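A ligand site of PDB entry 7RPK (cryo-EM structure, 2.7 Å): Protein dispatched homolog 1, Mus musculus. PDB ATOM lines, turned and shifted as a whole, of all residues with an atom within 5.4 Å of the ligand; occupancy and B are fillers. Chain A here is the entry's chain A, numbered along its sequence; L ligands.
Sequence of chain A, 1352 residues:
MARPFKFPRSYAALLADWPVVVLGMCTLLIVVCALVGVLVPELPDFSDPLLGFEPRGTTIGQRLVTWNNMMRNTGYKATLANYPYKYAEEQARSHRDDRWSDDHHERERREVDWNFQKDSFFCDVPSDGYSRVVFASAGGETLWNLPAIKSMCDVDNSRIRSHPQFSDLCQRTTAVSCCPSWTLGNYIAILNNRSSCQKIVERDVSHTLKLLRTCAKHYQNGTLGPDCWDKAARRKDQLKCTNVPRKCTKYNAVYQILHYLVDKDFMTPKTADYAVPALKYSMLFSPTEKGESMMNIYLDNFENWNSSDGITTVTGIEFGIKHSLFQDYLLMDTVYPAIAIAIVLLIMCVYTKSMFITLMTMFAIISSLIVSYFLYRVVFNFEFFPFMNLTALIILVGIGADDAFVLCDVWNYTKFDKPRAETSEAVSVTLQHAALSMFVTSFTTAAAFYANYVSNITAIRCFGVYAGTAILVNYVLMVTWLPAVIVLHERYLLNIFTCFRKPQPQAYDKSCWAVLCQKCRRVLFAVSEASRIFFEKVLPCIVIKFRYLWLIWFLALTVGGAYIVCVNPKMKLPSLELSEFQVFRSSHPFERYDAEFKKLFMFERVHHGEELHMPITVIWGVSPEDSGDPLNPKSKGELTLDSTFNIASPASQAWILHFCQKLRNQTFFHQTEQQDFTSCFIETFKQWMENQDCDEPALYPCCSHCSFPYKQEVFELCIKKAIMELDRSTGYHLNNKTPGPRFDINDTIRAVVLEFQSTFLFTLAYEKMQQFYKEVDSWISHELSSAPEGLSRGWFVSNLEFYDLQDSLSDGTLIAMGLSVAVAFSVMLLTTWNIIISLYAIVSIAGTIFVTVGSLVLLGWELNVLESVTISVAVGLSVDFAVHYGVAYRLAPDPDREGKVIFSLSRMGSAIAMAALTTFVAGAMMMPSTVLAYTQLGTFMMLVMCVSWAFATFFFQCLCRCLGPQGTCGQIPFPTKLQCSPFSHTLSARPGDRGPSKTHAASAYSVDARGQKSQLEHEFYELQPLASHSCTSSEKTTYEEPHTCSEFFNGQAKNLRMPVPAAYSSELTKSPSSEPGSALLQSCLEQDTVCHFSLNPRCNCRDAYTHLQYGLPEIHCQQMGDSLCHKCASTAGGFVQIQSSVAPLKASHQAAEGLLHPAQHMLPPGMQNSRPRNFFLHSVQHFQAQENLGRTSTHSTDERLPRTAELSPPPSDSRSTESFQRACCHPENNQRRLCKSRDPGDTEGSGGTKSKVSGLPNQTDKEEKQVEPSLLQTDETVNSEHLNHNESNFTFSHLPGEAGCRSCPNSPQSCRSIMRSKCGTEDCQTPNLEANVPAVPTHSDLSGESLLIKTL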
ATOM      1  N   GLN A 674      -2.563   7.576   9.090  1.00  0.00           N
ATOM      2  CA  GLN A 674      -2.137   8.045  10.413  1.00  0.00           C
ATOM      3  C   GLN A 674      -0.620   8.301  10.437  1.00  0.00           C
ATOM      4  O   GLN A 674       0.173   7.359  10.406  1.00  0.00           O
ATOM      5  CB  GLN A 674      -2.574   7.035  11.493  1.00  0.00           C
ATOM      6  CG  GLN A 674      -2.093   7.404  12.911  1.00  0.00           C
ATOM      7  CD  GLN A 674      -2.598   8.765  13.387  1.00  0.00           C
ATOM      8  OE1 GLN A 674      -3.790   9.014  13.487  1.00  0.00           O
ATOM      9  NE2 GLN A 674      -1.726   9.696  13.698  1.00  0.00           N
ATOM     10  N   GLN A 675      -0.208   9.565  10.534  1.00  0.00           N
ATOM     11  CA  GLN A 675       1.207   9.909  10.669  1.00  0.00           C
ATOM     12  C   GLN A 675       1.771   9.386  12.000  1.00  0.00           C
ATOM     13  O   GLN A 675       1.101   9.454  13.030  1.00  0.00           O
ATOM     14  CB  GLN A 675       1.363  11.436  10.516  1.00  0.00           C
ATOM     15  CG  GLN A 675       2.823  11.930  10.545  1.00  0.00           C
ATOM     16  CD  GLN A 675       3.698  11.266   9.476  1.00  0.00           C
ATOM     17  OE1 GLN A 675       4.202  10.169   9.657  1.00  0.00           O
ATOM     18  NE2 GLN A 675       3.878  11.880   8.331  1.00  0.00           N
ATOM     19  N   PHE A 677       4.899  10.388  14.295  1.00  0.00           N
ATOM     20  CA  PHE A 677       5.918  11.396  14.507  1.00  0.00           C
ATOM     21  C   PHE A 677       7.224  10.839  15.102  1.00  0.00           C
ATOM     22  O   PHE A 677       8.212  11.577  15.187  1.00  0.00           O
ATOM     23  CB  PHE A 677       5.284  12.534  15.315  1.00  0.00           C
ATOM     24  CG  PHE A 677       4.203  13.261  14.531  1.00  0.00           C
ATOM     25  CD1 PHE A 677       4.562  14.014  13.396  1.00  0.00           C
ATOM     26  CD2 PHE A 677       2.851  13.144  14.889  1.00  0.00           C
ATOM     27  CE1 PHE A 677       3.575  14.650  12.630  1.00  0.00           C
ATOM     28  CE2 PHE A 677       1.866  13.783  14.114  1.00  0.00           C
ATOM     29  CZ  PHE A 677       2.223  14.532  12.988  1.00  0.00           C
ATOM     30  N   THR A 678       7.298   9.557  15.473  1.00  0.00           N
ATOM     31  CA  THR A 678       8.570   8.902  15.779  1.00  0.00           C
ATOM     32  C   THR A 678       9.359   8.559  14.522  1.00  0.00           C
ATOM     33  O   THR A 678      10.583   8.671  14.530  1.00  0.00           O
ATOM     34  CB  THR A 678       8.382   7.607  16.559  1.00  0.00           C
ATOM     35  OG1 THR A 678       7.728   6.631  15.783  1.00  0.00           O
ATOM     36  CG2 THR A 678       7.598   7.727  17.860  1.00  0.00           C
ATOM     37  N   PHE A 681      12.374  11.250  12.830  1.00  0.00           N
ATOM     38  CA  PHE A 681      12.402  12.271  13.887  1.00  0.00           C
ATOM     39  C   PHE A 681      12.827  13.660  13.366  1.00  0.00           C
ATOM     40  O   PHE A 681      12.346  14.671  13.871  1.00  0.00           O
ATOM     41  CB  PHE A 681      13.279  11.785  15.052  1.00  0.00           C
ATOM     42  CG  PHE A 681      14.745  12.172  14.962  1.00  0.00           C
ATOM     43  CD1 PHE A 681      15.183  13.401  15.515  1.00  0.00           C
ATOM     44  CD2 PHE A 681      15.667  11.344  14.301  1.00  0.00           C
ATOM     45  CE1 PHE A 681      16.527  13.779  15.415  1.00  0.00           C
ATOM     46  CE2 PHE A 681      16.997  11.741  14.184  1.00  0.00           C
ATOM     47  CZ  PHE A 681      17.441  12.946  14.750  1.00  0.00           C
ATOM     48  N   ILE A 682      13.667  13.726  12.340  1.00  0.00           N
ATOM     49  CA  ILE A 682      14.118  14.980  11.715  1.00  0.00           C
ATOM     50  C   ILE A 682      12.963  15.786  11.100  1.00  0.00           C
ATOM     51  O   ILE A 682      12.958  17.008  11.195  1.00  0.00           O
ATOM     52  CB  ILE A 682      15.255  14.679  10.710  1.00  0.00           C
ATOM     53  CG1 ILE A 682      15.880  15.941  10.083  1.00  0.00           C
ATOM     54  CG2 ILE A 682      14.773  13.758   9.576  1.00  0.00           C
ATOM     55  CD1 ILE A 682      16.616  16.790  11.114  1.00  0.00           C
ATOM     56  N   THR A 684       9.651  15.597  12.222  1.00  0.00           N
ATOM     57  CA  THR A 684       8.937  16.077  13.397  1.00  0.00           C
ATOM     58  C   THR A 684       9.668  17.250  14.050  1.00  0.00           C
ATOM     59  O   THR A 684       9.039  18.247  14.416  1.00  0.00           O
ATOM     60  CB  THR A 684       8.768  14.955  14.416  1.00  0.00           C
ATOM     61  OG1 THR A 684       8.170  13.853  13.790  1.00  0.00           O
ATOM     62  CG2 THR A 684       7.874  15.342  15.590  1.00  0.00           C
ATOM     63  N   PHE A 685      10.997  17.202  14.128  1.00  0.00           N
ATOM     64  CA  PHE A 685      11.799  18.287  14.684  1.00  0.00           C
ATOM     65  C   PHE A 685      11.723  19.548  13.808  1.00  0.00           C
ATOM     66  O   PHE A 685      11.475  20.635  14.321  1.00  0.00           O
ATOM     67  CB  PHE A 685      13.239  17.812  14.869  1.00  0.00           C
ATOM     68  CG  PHE A 685      14.164  18.891  15.364  1.00  0.00           C
ATOM     69  CD1 PHE A 685      13.890  19.562  16.574  1.00  0.00           C
ATOM     70  CD2 PHE A 685      15.271  19.275  14.583  1.00  0.00           C
ATOM     71  CE1 PHE A 685      14.704  20.620  16.990  1.00  0.00           C
ATOM     72  CE2 PHE A 685      16.089  20.330  15.021  1.00  0.00           C
ATOM     73  CZ  PHE A 685      15.811  21.004  16.210  1.00  0.00           C
ATOM     74  N   LYS A 686      11.835  19.421  12.481  1.00  0.00           N
ATOM     75  CA  LYS A 686      11.639  20.523  11.535  1.00  0.00           C
ATOM     76  C   LYS A 686      10.258  21.167  11.696  1.00  0.00           C
ATOM     77  O   LYS A 686      10.146  22.384  11.796  1.00  0.00           O
ATOM     78  CB  LYS A 686      11.866  19.963  10.116  1.00  0.00           C
ATOM     79  CG  LYS A 686      11.667  20.981   8.991  1.00  0.00           C
ATOM     80  CD  LYS A 686      11.854  20.298   7.635  1.00  0.00           C
ATOM     81  CE  LYS A 686      11.798  21.272   6.448  1.00  0.00           C
ATOM     82  NZ  LYS A 686      10.449  21.863   6.254  1.00  0.00           N
ATOM     83  N   GLN A 687       9.198  20.366  11.823  1.00  0.00           N
ATOM     84  CA  GLN A 687       7.849  20.871  12.090  1.00  0.00           C
ATOM     85  C   GLN A 687       7.733  21.584  13.442  1.00  0.00           C
ATOM     86  O   GLN A 687       7.060  22.615  13.536  1.00  0.00           O
ATOM     87  CB  GLN A 687       6.852  19.710  12.053  1.00  0.00           C
ATOM     88  CG  GLN A 687       6.700  19.076  10.660  1.00  0.00           C
ATOM     89  CD  GLN A 687       5.985  17.727  10.701  1.00  0.00           C
ATOM     90  OE1 GLN A 687       5.416  17.317  11.694  1.00  0.00           O
ATOM     91  NE2 GLN A 687       5.968  16.999   9.598  1.00  0.00           N
ATOM     92  N   TRP A 688       8.379  21.067  14.485  1.00  0.00           N
ATOM     93  CA  TRP A 688       8.426  21.696  15.797  1.00  0.00           C
ATOM     94  C   TRP A 688       9.161  23.041  15.770  1.00  0.00           C
ATOM     95  O   TRP A 688       8.644  24.032  16.271  1.00  0.00           O
ATOM     96  CB  TRP A 688       9.059  20.746  16.828  1.00  0.00           C
ATOM     97  CG  TRP A 688       9.191  21.314  18.202  1.00  0.00           C
ATOM     98  CD1 TRP A 688       8.227  21.281  19.145  1.00  0.00           C
ATOM     99  CD2 TRP A 688      10.285  22.090  18.778  1.00  0.00           C
ATOM    100  NE1 TRP A 688       8.656  21.970  20.272  1.00  0.00           N
ATOM    101  CE2 TRP A 688       9.913  22.494  20.101  1.00  0.00           C
ATOM    102  CE3 TRP A 688      11.553  22.516  18.328  1.00  0.00           C
ATOM    103  CZ2 TRP A 688      10.744  23.266  20.913  1.00  0.00           C
ATOM    104  CZ3 TRP A 688      12.394  23.296  19.134  1.00  0.00           C
ATOM    105  CH2 TRP A 688      11.995  23.679  20.431  1.00  0.00           C
ATOM    106  N   GLU A 690       9.511  25.018  13.108  1.00  0.00           N
ATOM    107  CA  GLU A 690       8.600  25.915  12.377  1.00  0.00           C
ATOM    108  C   GLU A 690       7.399  26.402  13.211  1.00  0.00           C
ATOM    109  O   GLU A 690       6.802  27.412  12.841  1.00  0.00           O
ATOM    110  CB  GLU A 690       8.119  25.224  11.095  1.00  0.00           C
ATOM    111  CG  GLU A 690       9.232  25.135  10.048  1.00  0.00           C
ATOM    112  CD  GLU A 690       8.748  24.472   8.743  1.00  0.00           C
ATOM    113  OE1 GLU A 690       9.502  23.656   8.158  1.00  0.00           O
ATOM    114  OE2 GLU A 690       7.635  24.789   8.271  1.00  0.00           O
ATOM    115  N   ASN A 691       7.077  25.788  14.356  1.00  0.00           N
ATOM    116  CA  ASN A 691       6.046  26.294  15.270  1.00  0.00           C
ATOM    117  C   ASN A 691       6.540  27.404  16.218  1.00  0.00           C
ATOM    118  O   ASN A 691       5.712  28.073  16.836  1.00  0.00           O
ATOM    119  CB  ASN A 691       5.469  25.126  16.100  1.00  0.00           C
ATOM    120  CG  ASN A 691       4.332  24.432  15.392  1.00  0.00           C
ATOM    121  OD1 ASN A 691       3.191  24.865  15.446  1.00  0.00           O
ATOM    122  ND2 ASN A 691       4.587  23.343  14.725  1.00  0.00           N
ATOM    123  N   ILE A 719      17.404  20.295  19.523  1.00  0.00           N
ATOM    124  CA  ILE A 719      16.919  18.913  19.615  1.00  0.00           C
ATOM    125  C   ILE A 719      16.713  18.473  21.077  1.00  0.00           C
ATOM    126  O   ILE A 719      15.718  17.808  21.373  1.00  0.00           O
ATOM    127  CB  ILE A 719      17.833  17.949  18.820  1.00  0.00           C
ATOM    128  CG1 ILE A 719      17.267  16.528  18.701  1.00  0.00           C
ATOM    129  CG2 ILE A 719      19.224  17.824  19.455  1.00  0.00           C
ATOM    130  CD1 ILE A 719      15.887  16.451  18.042  1.00  0.00           C
ATOM    131  N   ALA A 722      13.454  20.371  22.302  1.00  0.00           N
ATOM    132  CA  ALA A 722      12.305  19.714  21.694  1.00  0.00           C
ATOM    133  C   ALA A 722      11.986  18.343  22.336  1.00  0.00           C
ATOM    134  O   ALA A 722      10.845  18.089  22.687  1.00  0.00           O
ATOM    135  CB  ALA A 722      12.578  19.596  20.199  1.00  0.00           C
ATOM    136  N   ILE A 723      12.991  17.484  22.553  1.00  0.00           N
ATOM    137  CA  ILE A 723      12.806  16.184  23.221  1.00  0.00           C
ATOM    138  C   ILE A 723      12.279  16.335  24.660  1.00  0.00           C
ATOM    139  O   ILE A 723      11.393  15.599  25.062  1.00  0.00           O
ATOM    140  CB  ILE A 723      14.123  15.370  23.153  1.00  0.00           C
ATOM    141  CG1 ILE A 723      14.418  14.862  21.737  1.00  0.00           C
ATOM    142  CG2 ILE A 723      14.151  14.204  24.145  1.00  0.00           C
ATOM    143  CD1 ILE A 723      13.572  13.667  21.270  1.00  0.00           C
ATOM    144  N   GLU A 725      10.563  19.075  25.776  1.00  0.00           N
ATOM    145  CA  GLU A 725       9.231  19.635  25.605  1.00  0.00           C
ATOM    146  C   GLU A 725       8.194  18.551  25.326  1.00  0.00           C
ATOM    147  O   GLU A 725       7.123  18.592  25.933  1.00  0.00           O
ATOM    148  CB  GLU A 725       9.207  20.718  24.526  1.00  0.00           C
ATOM    149  CG  GLU A 725       7.797  21.297  24.378  1.00  0.00           C
ATOM    150  CD  GLU A 725       7.792  22.627  23.623  1.00  0.00           C
ATOM    151  OE1 GLU A 725       8.409  23.603  24.093  1.00  0.00           O
ATOM    152  OE2 GLU A 725       7.144  22.698  22.553  1.00  0.00           O
ATOM    153  N   LEU A 726       8.500  17.548  24.496  1.00  0.00           N
ATOM    154  CA  LEU A 726       7.640  16.374  24.320  1.00  0.00           C
ATOM    155  C   LEU A 726       7.371  15.689  25.669  1.00  0.00           C
ATOM    156  O   LEU A 726       6.215  15.460  26.027  1.00  0.00           O
ATOM    157  CB  LEU A 726       8.320  15.411  23.318  1.00  0.00           C
ATOM    158  CG  LEU A 726       7.691  14.014  23.238  1.00  0.00           C
ATOM    159  CD1 LEU A 726       6.303  14.057  22.603  1.00  0.00           C
ATOM    160  CD2 LEU A 726       8.585  13.093  22.412  1.00  0.00           C
ATOM    161  N   THR A 730       3.379  15.977  26.936  1.00  0.00           N
ATOM    162  CA  THR A 730       2.573  14.865  26.423  1.00  0.00           C
ATOM    163  C   THR A 730       2.717  13.596  27.257  1.00  0.00           C
ATOM    164  O   THR A 730       3.815  13.217  27.667  1.00  0.00           O
ATOM    165  CB  THR A 730       2.937  14.594  24.942  1.00  0.00           C
ATOM    166  OG1 THR A 730       2.809  15.780  24.189  1.00  0.00           O
ATOM    167  CG2 THR A 730       2.037  13.564  24.275  1.00  0.00           C
ATOM    168  N   TYR A 732       3.198  10.601  26.602  1.00  0.00           N
ATOM    169  CA  TYR A 732       3.826   9.659  25.673  1.00  0.00           C
ATOM    170  C   TYR A 732       5.312   9.488  26.024  1.00  0.00           C
ATOM    171  O   TYR A 732       6.000  10.462  26.300  1.00  0.00           O
ATOM    172  CB  TYR A 732       3.662  10.184  24.237  1.00  0.00           C
ATOM    173  CG  TYR A 732       4.224   9.259  23.189  1.00  0.00           C
ATOM    174  CD1 TYR A 732       3.402   8.269  22.633  1.00  0.00           C
ATOM    175  CD2 TYR A 732       5.566   9.374  22.774  1.00  0.00           C
ATOM    176  CE1 TYR A 732       3.913   7.389  21.658  1.00  0.00           C
ATOM    177  CE2 TYR A 732       6.081   8.507  21.804  1.00  0.00           C
ATOM    178  CZ  TYR A 732       5.250   7.512  21.244  1.00  0.00           C
ATOM    179  OH  TYR A 732       5.732   6.652  20.314  1.00  0.00           O
ATOM    180  N   LEU A 734       9.303   7.510  25.510  1.00  0.00           N
ATOM    181  CA  LEU A 734      10.314   6.932  24.639  1.00  0.00           C
ATOM    182  C   LEU A 734      10.990   5.776  25.377  1.00  0.00           C
ATOM    183  O   LEU A 734      11.420   5.926  26.518  1.00  0.00           O
ATOM    184  CB  LEU A 734      11.335   8.017  24.254  1.00  0.00           C
ATOM    185  CG  LEU A 734      10.759   9.334  23.714  1.00  0.00           C
ATOM    186  CD1 LEU A 734      11.874  10.313  23.396  1.00  0.00           C
ATOM    187  CD2 LEU A 734       9.937   9.115  22.455  1.00  0.00           C
ATOM    188  N   PRO A 739      11.995   4.836  17.777  1.00  0.00           N
ATOM    189  CA  PRO A 739      12.866   5.602  16.875  1.00  0.00           C
ATOM    190  C   PRO A 739      13.251   6.972  17.450  1.00  0.00           C
ATOM    191  O   PRO A 739      12.551   7.528  18.284  1.00  0.00           O
ATOM    192  CB  PRO A 739      12.077   5.744  15.581  1.00  0.00           C
ATOM    193  CG  PRO A 739      11.114   4.573  15.615  1.00  0.00           C
ATOM    194  CD  PRO A 739      10.778   4.472  17.084  1.00  0.00           C
ATOM    195  N   GLY A 740      14.359   7.545  16.989  1.00  0.00           N
ATOM    196  CA  GLY A 740      14.852   8.847  17.440  1.00  0.00           C
ATOM    197  C   GLY A 740      16.355   8.890  17.650  1.00  0.00           C
ATOM    198  O   GLY A 740      17.048   7.907  17.370  1.00  0.00           O
ATOM    199  N   PRO A 741      16.910  10.019  18.123  1.00  0.00           N
ATOM    200  CA  PRO A 741      18.300  10.113  18.515  1.00  0.00           C
ATOM    201  C   PRO A 741      18.586   9.291  19.772  1.00  0.00           C
ATOM    202  O   PRO A 741      17.706   9.042  20.592  1.00  0.00           O
ATOM    203  CB  PRO A 741      18.549  11.604  18.743  1.00  0.00           C
ATOM    204  CG  PRO A 741      17.189  12.108  19.206  1.00  0.00           C
ATOM    205  CD  PRO A 741      16.210  11.255  18.415  1.00  0.00           C
HETATM  206  C1  LIG L   1       2.839  18.351  16.543  1.00  0.00           C
HETATM  207  O1  LIG L   1       2.199  17.459  17.491  1.00  0.00           O
HETATM  208  C2  LIG L   1       2.909  17.741  15.101  1.00  0.00           C
HETATM  209  O2  LIG L   1       3.873  16.666  15.012  1.00  0.00           O
HETATM  210  C3  LIG L   1       3.311  18.816  14.061  1.00  0.00           C
HETATM  211  O3  LIG L   1       3.165  18.311  12.732  1.00  0.00           O
HETATM  212  C4  LIG L   1       2.523  20.131  14.222  1.00  0.00           C
HETATM  213  O4  LIG L   1       3.202  21.108  13.394  1.00  0.00           O
HETATM  214  C5  LIG L   1       2.508  20.622  15.695  1.00  0.00           C
HETATM  215  O5  LIG L   1       2.010  19.528  16.506  1.00  0.00           O
HETATM  216  C6  LIG L   1       1.578  21.845  15.929  1.00  0.00           C
HETATM  217  O6  LIG L   1       0.202  21.489  15.744  1.00  0.00           O
HETATM  218  C7  LIG L   1      11.468  14.977  17.033  1.00  0.00           C
HETATM  219  C8  LIG L   1      11.806  11.327  18.827  1.00  0.00           C
HETATM  220  O7  LIG L   1       0.349  24.633  11.520  1.00  0.00           O
HETATM  221  O8  LIG L   1      -0.484   7.394  16.939  1.00  0.00           O
HETATM  222  O9  LIG L   1      -0.565  11.375  20.895  1.00  0.00           O
HETATM  223  O10 LIG L   1      -2.761  12.169  15.129  1.00  0.00           O
HETATM  224  O11 LIG L   1      -1.608  14.743  15.617  1.00  0.00           O
HETATM  225  O12 LIG L   1       5.177  24.579  12.107  1.00  0.00           O
HETATM  226  O13 LIG L   1      -4.045   6.398  19.332  1.00  0.00           O
HETATM  227  O14 LIG L   1       5.345  22.299   9.958  1.00  0.00           O
HETATM  228  O15 LIG L   1      -6.486   7.653  18.480  1.00  0.00           O
HETATM  229  O16 LIG L   1       3.600  20.238  10.798  1.00  0.00           O
HETATM  230  O17 LIG L   1      -6.171  10.232  17.188  1.00  0.00           O
HETATM  231  C9  LIG L   1      11.907  15.540  18.388  1.00  0.00           C
HETATM  232  C10 LIG L   1      10.467  11.998  18.491  1.00  0.00           C
HETATM  233  C11 LIG L   1      10.998  16.681  18.891  1.00  0.00           C
HETATM  234  C12 LIG L   1       9.273  11.215  19.057  1.00  0.00           C
HETATM  235  C13 LIG L   1       9.534  16.266  19.091  1.00  0.00           C
HETATM  236  C14 LIG L   1       7.913  11.919  18.817  1.00  0.00           C
HETATM  237  C15 LIG L   1       8.676  17.404  19.671  1.00  0.00           C
HETATM  238  C16 LIG L   1       6.772  11.186  19.537  1.00  0.00           C
HETATM  239  C17 LIG L   1       7.175  17.064  19.595  1.00  0.00           C
HETATM  240  C18 LIG L   1       5.422  11.912  19.418  1.00  0.00           C
HETATM  241  C19 LIG L   1       6.311  17.982  20.494  1.00  0.00           C
HETATM  242  C20 LIG L   1       4.357  11.267  20.335  1.00  0.00           C
HETATM  243  C21 LIG L   1       4.784  17.848  20.219  1.00  0.00           C
HETATM  244  C22 LIG L   1       2.902  11.724  20.095  1.00  0.00           C
HETATM  245  C23 LIG L   1       4.224  16.455  20.587  1.00  0.00           C
HETATM  246  C24 LIG L   1       2.672  13.251  20.293  1.00  0.00           C
HETATM  247  C25 LIG L   1       1.622  24.486  10.862  1.00  0.00           C
HETATM  248  C26 LIG L   1      -1.638   6.757  17.496  1.00  0.00           C
HETATM  249  C27 LIG L   1      -1.240  10.818  19.754  1.00  0.00           C
HETATM  250  C28 LIG L   1       2.698  16.315  20.288  1.00  0.00           C
HETATM  251  C29 LIG L   1       2.864  14.058  18.987  1.00  0.00           C
HETATM  252  C30 LIG L   1       2.855  16.200  17.720  1.00  0.00           C
HETATM  253  C31 LIG L   1       0.733  15.473  18.932  1.00  0.00           C
HETATM  254  O18 LIG L   1       0.323  14.776  17.741  1.00  0.00           O
HETATM  255  O19 LIG L   1      -0.593  12.838  18.612  1.00  0.00           O
HETATM  256  O20 LIG L   1       2.375  23.149  12.802  1.00  0.00           O
HETATM  257  O21 LIG L   1      -2.875   8.616  16.593  1.00  0.00           O
HETATM  258  O22 LIG L   1      -3.415  10.650  17.684  1.00  0.00           O
HETATM  259  C32 LIG L   1       2.746  24.238  11.904  1.00  0.00           C
HETATM  260  C33 LIG L   1      -2.740   7.816  17.790  1.00  0.00           C
HETATM  261  C34 LIG L   1      -1.723  11.961  18.824  1.00  0.00           C
HETATM  262  C35 LIG L   1      -2.509  12.615  16.470  1.00  0.00           C
HETATM  263  C36 LIG L   1      -0.891  14.028  17.865  1.00  0.00           C
HETATM  264  C37 LIG L   1      -1.311  13.592  16.434  1.00  0.00           C
HETATM  265  C38 LIG L   1       2.294  15.516  19.002  1.00  0.00           C
HETATM  266  C39 LIG L   1       4.166  23.988  11.293  1.00  0.00           C
HETATM  267  C40 LIG L   1      -4.112   7.171  18.117  1.00  0.00           C
HETATM  268  C41 LIG L   1      -2.212  11.422  17.446  1.00  0.00           C
HETATM  269  C42 LIG L   1       2.435  21.764  12.368  1.00  0.00           C
HETATM  270  C43 LIG L   1      -3.827   9.718  16.651  1.00  0.00           C
HETATM  271  C44 LIG L   1       4.511  22.475  11.116  1.00  0.00           C
HETATM  272  C45 LIG L   1      -5.195   8.268  18.265  1.00  0.00           C
HETATM  273  C46 LIG L   1       3.248  21.610  11.038  1.00  0.00           C
HETATM  274  C47 LIG L   1      -5.239   9.165  16.996  1.00  0.00           C
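The backbone carbonyl oxygen (O) of Gln 687 lies within hydrogen-bond range of the side-chain amide nitrogen (ND2) of Asn 691 (2.8 Å). The side-chain carboxylate of Glu 690 is in salt-bridge range of the side-chain amino group of Lys 686 (2.8 Å). The backbone carbonyl oxygen (O) of Phe 677 lies within hydrogen-bond range of the side-chain hydroxyl (OG1) of Thr 684 (2.7 Å). The indole nitrogen (NE1) of Trp 688 is in hydrogen-bond range of the side-chain carboxylate (OE2) of Glu 725 (2.8 Å).
Phe 677 touches the ligand (CE1 to O2, 3.1 Å). Thr 678 touches the ligand (CG2 to C16, 3.9 Å). Phe 681 touches the ligand (O to C7, 3.3 Å). CB of Thr 684 touches C7 of the ligand (3.8 Å). Phe 685 touches the ligand (N to C7, 3.7 Å). CD1 of Trp 688 touches C15 of the ligand (3.9 Å). Ala 722 touches the ligand. Ile 723 touches the ligand (CD1 to C8, 3.8 Å). Leu 726 touches the ligand (CD1 to C23, 3.8 Å). Thr 730 touches the ligand. Tyr 732 touches the ligand (CD2 to C20, 3.3 Å). Pro 739 touches the ligand (O to C8, 3.9 Å). Hydrophobic or aromatic side chains that line the ligand: Phe 677, Phe 685, Trp 688, Ala 722, Ile 723, Leu 726 and Tyr 732. Of the 24 residues printed, 16 come within 4 Å of the ligand.
O12 of the ligand sits at hydrogen-bond distance from O of Gln 687 (3.1 Å). An oxygen (O3) of the ligand sits at hydrogen-bond distance from the side-chain amide oxygen (OE1) of Gln 687 (2.7 Å). O12 of the ligand lies within hydrogen-bond range of N of Asn 691 (3.2 Å). An oxygen (O20) of the ligand is in hydrogen-bond range of the side-chain amide nitrogen of Asn 691 (2.9 Å). The side-chain amide nitrogen of Gln 674 sits at hydrogen-bond distance from an oxygen (O10) of the ligand (3.0 Å). O of Glu 690 lies close to O12 of the ligand (3.3 Å).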
